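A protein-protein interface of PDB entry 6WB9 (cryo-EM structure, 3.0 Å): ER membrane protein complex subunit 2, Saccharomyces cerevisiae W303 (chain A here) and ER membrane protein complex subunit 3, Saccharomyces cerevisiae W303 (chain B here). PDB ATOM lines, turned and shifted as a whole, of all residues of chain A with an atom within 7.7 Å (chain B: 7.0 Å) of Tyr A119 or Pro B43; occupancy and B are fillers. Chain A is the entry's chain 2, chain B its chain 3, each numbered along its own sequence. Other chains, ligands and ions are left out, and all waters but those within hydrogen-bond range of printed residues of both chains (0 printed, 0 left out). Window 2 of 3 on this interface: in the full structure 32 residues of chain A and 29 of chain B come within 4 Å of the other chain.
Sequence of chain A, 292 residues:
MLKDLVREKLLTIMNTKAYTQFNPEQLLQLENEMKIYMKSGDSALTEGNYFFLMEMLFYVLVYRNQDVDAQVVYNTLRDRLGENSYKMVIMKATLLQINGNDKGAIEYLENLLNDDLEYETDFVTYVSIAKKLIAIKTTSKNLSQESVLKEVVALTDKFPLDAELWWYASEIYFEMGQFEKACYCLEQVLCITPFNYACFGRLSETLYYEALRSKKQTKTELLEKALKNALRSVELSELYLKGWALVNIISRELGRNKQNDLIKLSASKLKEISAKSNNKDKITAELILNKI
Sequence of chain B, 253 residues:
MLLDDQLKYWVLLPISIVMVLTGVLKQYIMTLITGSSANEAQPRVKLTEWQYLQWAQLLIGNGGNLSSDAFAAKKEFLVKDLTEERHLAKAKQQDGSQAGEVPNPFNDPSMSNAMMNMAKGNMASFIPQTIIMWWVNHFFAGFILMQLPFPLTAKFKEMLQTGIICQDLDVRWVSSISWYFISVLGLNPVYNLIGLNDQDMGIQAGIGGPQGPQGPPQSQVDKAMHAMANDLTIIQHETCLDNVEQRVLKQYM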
ATOM      1  N   ASP A 115      23.247   5.342   2.450  1.00  0.00           N
ATOM      2  CA  ASP A 115      21.917   4.742   2.467  1.00  0.00           C
ATOM      3  C   ASP A 115      21.846   3.509   1.566  1.00  0.00           C
ATOM      4  O   ASP A 115      21.097   2.569   1.863  1.00  0.00           O
ATOM      5  CB  ASP A 115      20.876   5.790   2.055  1.00  0.00           C
ATOM      6  CG  ASP A 115      19.526   5.185   1.706  1.00  0.00           C
ATOM      7  OD1 ASP A 115      18.933   4.504   2.569  1.00  0.00           O
ATOM      8  OD2 ASP A 115      19.059   5.394   0.567  1.00  0.00           O
ATOM      9  N   ASP A 116      22.648   3.465   0.494  1.00  0.00           N
ATOM     10  CA  ASP A 116      22.647   2.348  -0.445  1.00  0.00           C
ATOM     11  C   ASP A 116      23.690   1.288  -0.115  1.00  0.00           C
ATOM     12  O   ASP A 116      24.247   0.670  -1.029  1.00  0.00           O
ATOM     13  CB  ASP A 116      22.856   2.841  -1.879  1.00  0.00           C
ATOM     14  CG  ASP A 116      21.555   3.069  -2.617  1.00  0.00           C
ATOM     15  OD1 ASP A 116      20.489   2.707  -2.079  1.00  0.00           O
ATOM     16  OD2 ASP A 116      21.597   3.610  -3.741  1.00  0.00           O
ATOM     17  N   LEU A 117      23.990   1.069   1.159  1.00  0.00           N
ATOM     18  CA  LEU A 117      24.842  -0.042   1.558  1.00  0.00           C
ATOM     19  C   LEU A 117      24.048  -1.171   2.194  1.00  0.00           C
ATOM     20  O   LEU A 117      24.169  -2.328   1.778  1.00  0.00           O
ATOM     21  CB  LEU A 117      25.930   0.441   2.528  1.00  0.00           C
ATOM     22  CG  LEU A 117      27.112  -0.510   2.720  1.00  0.00           C
ATOM     23  CD1 LEU A 117      28.041  -0.461   1.515  1.00  0.00           C
ATOM     24  CD2 LEU A 117      27.867  -0.190   4.001  1.00  0.00           C
ATOM     25  N   GLU A 118      23.226  -0.858   3.190  1.00  0.00           N
ATOM     26  CA  GLU A 118      22.405  -1.842   3.881  1.00  0.00           C
ATOM     27  C   GLU A 118      20.979  -1.761   3.358  1.00  0.00           C
ATOM     28  O   GLU A 118      20.446  -0.658   3.181  1.00  0.00           O
ATOM     29  CB  GLU A 118      22.425  -1.612   5.394  1.00  0.00           C
ATOM     30  CG  GLU A 118      23.815  -1.500   6.005  1.00  0.00           C
ATOM     31  CD  GLU A 118      24.309  -0.067   6.080  1.00  0.00           C
ATOM     32  OE1 GLU A 118      23.527   0.849   5.747  1.00  0.00           O
ATOM     33  OE2 GLU A 118      25.477   0.142   6.466  1.00  0.00           O
ATOM     34  N   TYR A 119      20.380  -2.936   3.108  1.00  0.00           N
ATOM     35  CA  TYR A 119      18.995  -3.091   2.634  1.00  0.00           C
ATOM     36  C   TYR A 119      18.773  -2.360   1.310  1.00  0.00           C
ATOM     37  O   TYR A 119      17.733  -1.740   1.082  1.00  0.00           O
ATOM     38  CB  TYR A 119      17.983  -2.645   3.695  1.00  0.00           C
ATOM     39  CG  TYR A 119      18.193  -3.301   5.044  1.00  0.00           C
ATOM     40  CD1 TYR A 119      18.488  -4.659   5.143  1.00  0.00           C
ATOM     41  CD2 TYR A 119      18.111  -2.561   6.219  1.00  0.00           C
ATOM     42  CE1 TYR A 119      18.689  -5.262   6.372  1.00  0.00           C
ATOM     43  CE2 TYR A 119      18.311  -3.156   7.456  1.00  0.00           C
ATOM     44  CZ  TYR A 119      18.599  -4.506   7.524  1.00  0.00           C
ATOM     45  OH  TYR A 119      18.797  -5.101   8.748  1.00  0.00           O
ATOM     46  N   GLU A 120      19.769  -2.444   0.434  1.00  0.00           N
ATOM     47  CA  GLU A 120      19.778  -1.741  -0.837  1.00  0.00           C
ATOM     48  C   GLU A 120      18.816  -2.406  -1.827  1.00  0.00           C
ATOM     49  O   GLU A 120      18.290  -3.497  -1.597  1.00  0.00           O
ATOM     50  CB  GLU A 120      21.204  -1.722  -1.399  1.00  0.00           C
ATOM     51  CG  GLU A 120      21.418  -0.962  -2.699  1.00  0.00           C
ATOM     52  CD  GLU A 120      22.863  -0.966  -3.136  1.00  0.00           C
ATOM     53  OE1 GLU A 120      23.693  -1.593  -2.445  1.00  0.00           O
ATOM     54  OE2 GLU A 120      23.167  -0.354  -4.180  1.00  0.00           O
ATOM     55  N   THR A 121      18.590  -1.716  -2.946  1.00  0.00           N
ATOM     56  CA  THR A 121      18.009  -2.273  -4.161  1.00  0.00           C
ATOM     57  C   THR A 121      19.073  -3.033  -4.950  1.00  0.00           C
ATOM     58  O   THR A 121      20.110  -3.416  -4.399  1.00  0.00           O
ATOM     59  CB  THR A 121      17.388  -1.167  -5.019  1.00  0.00           C
ATOM     60  OG1 THR A 121      18.326  -0.096  -5.179  1.00  0.00           O
ATOM     61  CG2 THR A 121      16.122  -0.634  -4.368  1.00  0.00           C
ATOM     62  N   ASP A 122      18.805  -3.279  -6.233  1.00  0.00           N
ATOM     63  CA  ASP A 122      19.642  -4.117  -7.084  1.00  0.00           C
ATOM     64  C   ASP A 122      21.033  -3.511  -7.299  1.00  0.00           C
ATOM     65  O   ASP A 122      21.333  -2.385  -6.893  1.00  0.00           O
ATOM     66  CB  ASP A 122      18.962  -4.334  -8.433  1.00  0.00           C
ATOM     67  CG  ASP A 122      18.666  -3.033  -9.145  1.00  0.00           C
ATOM     68  OD1 ASP A 122      18.471  -2.009  -8.456  1.00  0.00           O
ATOM     69  OD2 ASP A 122      18.633  -3.032 -10.392  1.00  0.00           O
ATOM     70  N   PHE A 123      21.889  -4.284  -7.973  1.00  0.00           N
ATOM     71  CA  PHE A 123      23.297  -3.919  -8.081  1.00  0.00           C
ATOM     72  C   PHE A 123      23.521  -2.795  -9.086  1.00  0.00           C
ATOM     73  O   PHE A 123      24.520  -2.071  -8.982  1.00  0.00           O
ATOM     74  CB  PHE A 123      24.125  -5.166  -8.429  1.00  0.00           C
ATOM     75  CG  PHE A 123      24.652  -5.205  -9.844  1.00  0.00           C
ATOM     76  CD1 PHE A 123      23.864  -5.681 -10.880  1.00  0.00           C
ATOM     77  CD2 PHE A 123      25.960  -4.827 -10.125  1.00  0.00           C
ATOM     78  CE1 PHE A 123      24.353  -5.737 -12.174  1.00  0.00           C
ATOM     79  CE2 PHE A 123      26.453  -4.877 -11.416  1.00  0.00           C
ATOM     80  CZ  PHE A 123      25.651  -5.336 -12.439  1.00  0.00           C
ATOM     81  N   PHE A 159      31.831  -5.525  -5.986  1.00  0.00           N
ATOM     82  CA  PHE A 159      31.038  -5.418  -7.212  1.00  0.00           C
ATOM     83  C   PHE A 159      31.814  -5.687  -8.502  1.00  0.00           C
ATOM     84  O   PHE A 159      32.058  -4.749  -9.273  1.00  0.00           O
ATOM     85  CB  PHE A 159      30.396  -4.030  -7.308  1.00  0.00           C
ATOM     86  CG  PHE A 159      29.004  -3.968  -6.770  1.00  0.00           C
ATOM     87  CD1 PHE A 159      28.684  -4.560  -5.562  1.00  0.00           C
ATOM     88  CD2 PHE A 159      28.018  -3.302  -7.467  1.00  0.00           C
ATOM     89  CE1 PHE A 159      27.398  -4.501  -5.069  1.00  0.00           C
ATOM     90  CE2 PHE A 159      26.737  -3.235  -6.976  1.00  0.00           C
ATOM     91  CZ  PHE A 159      26.425  -3.836  -5.776  1.00  0.00           C
ATOM     92  N   ALA B  41      16.305  -6.995  -4.174  1.00  0.00           N
ATOM     93  CA  ALA B  41      16.735  -5.888  -3.324  1.00  0.00           C
ATOM     94  C   ALA B  41      17.477  -6.474  -2.127  1.00  0.00           C
ATOM     95  O   ALA B  41      16.862  -6.881  -1.139  1.00  0.00           O
ATOM     96  CB  ALA B  41      15.545  -5.040  -2.888  1.00  0.00           C
ATOM     97  N   GLN B  42      18.799  -6.511  -2.221  1.00  0.00           N
ATOM     98  CA  GLN B  42      19.683  -7.080  -1.219  1.00  0.00           C
ATOM     99  C   GLN B  42      20.691  -6.030  -0.769  1.00  0.00           C
ATOM    100  O   GLN B  42      20.893  -5.023  -1.458  1.00  0.00           O
ATOM    101  CB  GLN B  42      20.420  -8.301  -1.790  1.00  0.00           C
ATOM    102  CG  GLN B  42      19.507  -9.386  -2.326  1.00  0.00           C
ATOM    103  CD  GLN B  42      20.277 -10.564  -2.883  1.00  0.00           C
ATOM    104  OE1 GLN B  42      21.448 -10.762  -2.565  1.00  0.00           O
ATOM    105  NE2 GLN B  42      19.623 -11.354  -3.725  1.00  0.00           N
ATOM    106  N   PRO B  43      21.335  -6.219   0.385  1.00  0.00           N
ATOM    107  CA  PRO B  43      22.463  -5.351   0.749  1.00  0.00           C
ATOM    108  C   PRO B  43      23.671  -5.595  -0.146  1.00  0.00           C
ATOM    109  O   PRO B  43      23.717  -6.528  -0.950  1.00  0.00           O
ATOM    110  CB  PRO B  43      22.757  -5.732   2.201  1.00  0.00           C
ATOM    111  CG  PRO B  43      21.471  -6.269   2.711  1.00  0.00           C
ATOM    112  CD  PRO B  43      20.853  -6.987   1.548  1.00  0.00           C
ATOM    113  N   ARG B  44      24.680  -4.737   0.035  1.00  0.00           N
ATOM    114  CA  ARG B  44      25.797  -4.668  -0.906  1.00  0.00           C
ATOM    115  C   ARG B  44      26.700  -5.894  -0.814  1.00  0.00           C
ATOM    116  O   ARG B  44      27.246  -6.339  -1.829  1.00  0.00           O
ATOM    117  CB  ARG B  44      26.598  -3.388  -0.659  1.00  0.00           C
ATOM    118  CG  ARG B  44      27.467  -2.929  -1.825  1.00  0.00           C
ATOM    119  CD  ARG B  44      28.912  -3.382  -1.677  1.00  0.00           C
ATOM    120  NE  ARG B  44      29.507  -2.902  -0.437  1.00  0.00           N
ATOM    121  CZ  ARG B  44      30.585  -3.432   0.128  1.00  0.00           C
ATOM    122  NH1 ARG B  44      31.186  -4.470  -0.434  1.00  0.00           N
ATOM    123  NH2 ARG B  44      31.059  -2.929   1.258  1.00  0.00           N
ATOM    124  N   VAL B  45      26.874  -6.451   0.385  1.00  0.00           N
ATOM    125  CA  VAL B  45      27.812  -7.559   0.549  1.00  0.00           C
ATOM    126  C   VAL B  45      27.234  -8.856  -0.009  1.00  0.00           C
ATOM    127  O   VAL B  45      27.977  -9.687  -0.551  1.00  0.00           O
ATOM    128  CB  VAL B  45      28.205  -7.706   2.028  1.00  0.00           C
ATOM    129  CG1 VAL B  45      29.486  -8.514   2.160  1.00  0.00           C
ATOM    130  CG2 VAL B  45      28.369  -6.339   2.669  1.00  0.00           C
ATOM    131  N   LYS B  46      25.914  -9.043   0.092  1.00  0.00           N
ATOM    132  CA  LYS B  46      25.270 -10.183  -0.551  1.00  0.00           C
ATOM    133  C   LYS B  46      25.357 -10.077  -2.069  1.00  0.00           C
ATOM    134  O   LYS B  46      25.576 -11.083  -2.756  1.00  0.00           O
ATOM    135  CB  LYS B  46      23.812 -10.283  -0.105  1.00  0.00           C
ATOM    136  CG  LYS B  46      23.628 -10.386   1.398  1.00  0.00           C
ATOM    137  CD  LYS B  46      24.319 -11.617   1.960  1.00  0.00           C
ATOM    138  CE  LYS B  46      24.158 -11.696   3.471  1.00  0.00           C
ATOM    139  NZ  LYS B  46      24.904 -12.847   4.054  1.00  0.00           N
ATOM    140  N   LEU B  47      25.215  -8.858  -2.601  1.00  0.00           N
ATOM    141  CA  LEU B  47      25.404  -8.628  -4.029  1.00  0.00           C
ATOM    142  C   LEU B  47      26.842  -8.879  -4.457  1.00  0.00           C
ATOM    143  O   LEU B  47      27.070  -9.398  -5.550  1.00  0.00           O
ATOM    144  CB  LEU B  47      24.991  -7.203  -4.396  1.00  0.00           C
ATOM    145  CG  LEU B  47      23.505  -6.872  -4.277  1.00  0.00           C
ATOM    146  CD1 LEU B  47      23.261  -5.401  -4.557  1.00  0.00           C
ATOM    147  CD2 LEU B  47      22.688  -7.743  -5.211  1.00  0.00           C
ATOM    148  N   THR B  48      27.815  -8.564  -3.600  1.00  0.00           N
ATOM    149  CA  THR B  48      29.214  -8.811  -3.944  1.00  0.00           C
ATOM    150  C   THR B  48      29.538 -10.302  -3.931  1.00  0.00           C
ATOM    151  O   THR B  48      30.245 -10.797  -4.820  1.00  0.00           O
ATOM    152  CB  THR B  48      30.128  -8.046  -2.986  1.00  0.00           C
ATOM    153  OG1 THR B  48      29.767  -6.661  -2.988  1.00  0.00           O
ATOM    154  CG2 THR B  48      31.579  -8.172  -3.410  1.00  0.00           C
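OE1 of Glu A120 lies close to O of Asp A116, at 2.7 Å.
The backbone carbonyl oxygen (O) of Arg B44 sits at hydrogen-bond distance from the side-chain hydroxyl (OG1) of Thr B48 (2.8 Å).
N of Arg B44 is in hydrogen-bond range of O of Leu A117, at 3.0 Å.
The backbone carbonyl oxygen (O) of Glu A120 lies within hydrogen-bond range of the backbone NH (N) of Gln B42, 3.1 Å away.
The backbone carbonyl oxygen (O) of Gln B42 sits close to the backbone carbonyl oxygen (O) of Thr A121 (3.4 Å).
Of the 8 printed residues of chain B, 6 touch a printed residue of chain A.
Printed residues of chain B that touch a printed residue of chain A: Ala B41, Gln B42, Pro B43, Arg B44, Leu B47 and Thr B48.
Hydrophobic or aromatic side chains of chain B that line the printed part of chain A: Ala B41, Pro B43 and Leu B47.
Of the 10 printed residues of chain A, 6 touch a printed residue of chain B.
Among the printed residues, merely in contact across the chains: Glu A120 with Ala B41, Phe A159 with Thr B48, Tyr A119 with Pro B43, Phe A159 with Arg B44, Leu A117 with Pro B43, Phe A159 with Leu B47, Thr A121 with Leu B47, Phe A123 with Leu B47, Glu A120 with Arg B44, Thr A121 with Ala B41 and Glu A120 with Pro B43.
Tyr A119 touches one residue of chain B.
Pro B43 touches just these residues of chain A: Leu A117, Tyr A119 and Glu A120.
Printed residues of chain A within 4 Å of Thr B48: Phe A159.
Printed residues of chain B within 4 Å of Thr A121: Ala B41 (3.9 Å), Gln B42 (3.4 Å) and Leu B47 (3.7 Å).
Of the printed residues of chain B, Glu A120 touches Ala B41 (3.1 Å), Gln B42 (3.0 Å), Pro B43 (3.98 Å) and Arg B44 (3.9 Å).
Of the printed residues of chain A, Ala B41 touches Glu A120 (3.1 Å) and Thr A121 (3.9 Å).
Printed residues of chain B within 4 Å of Phe A123: Leu B47.
Asp A115 touches none of the printed residues of chain B.
Lys B46 touches none of the printed residues of chain A.
The nearest residue of chain A that does not touch Pro B43 is Glu A118 (4.3 Å).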
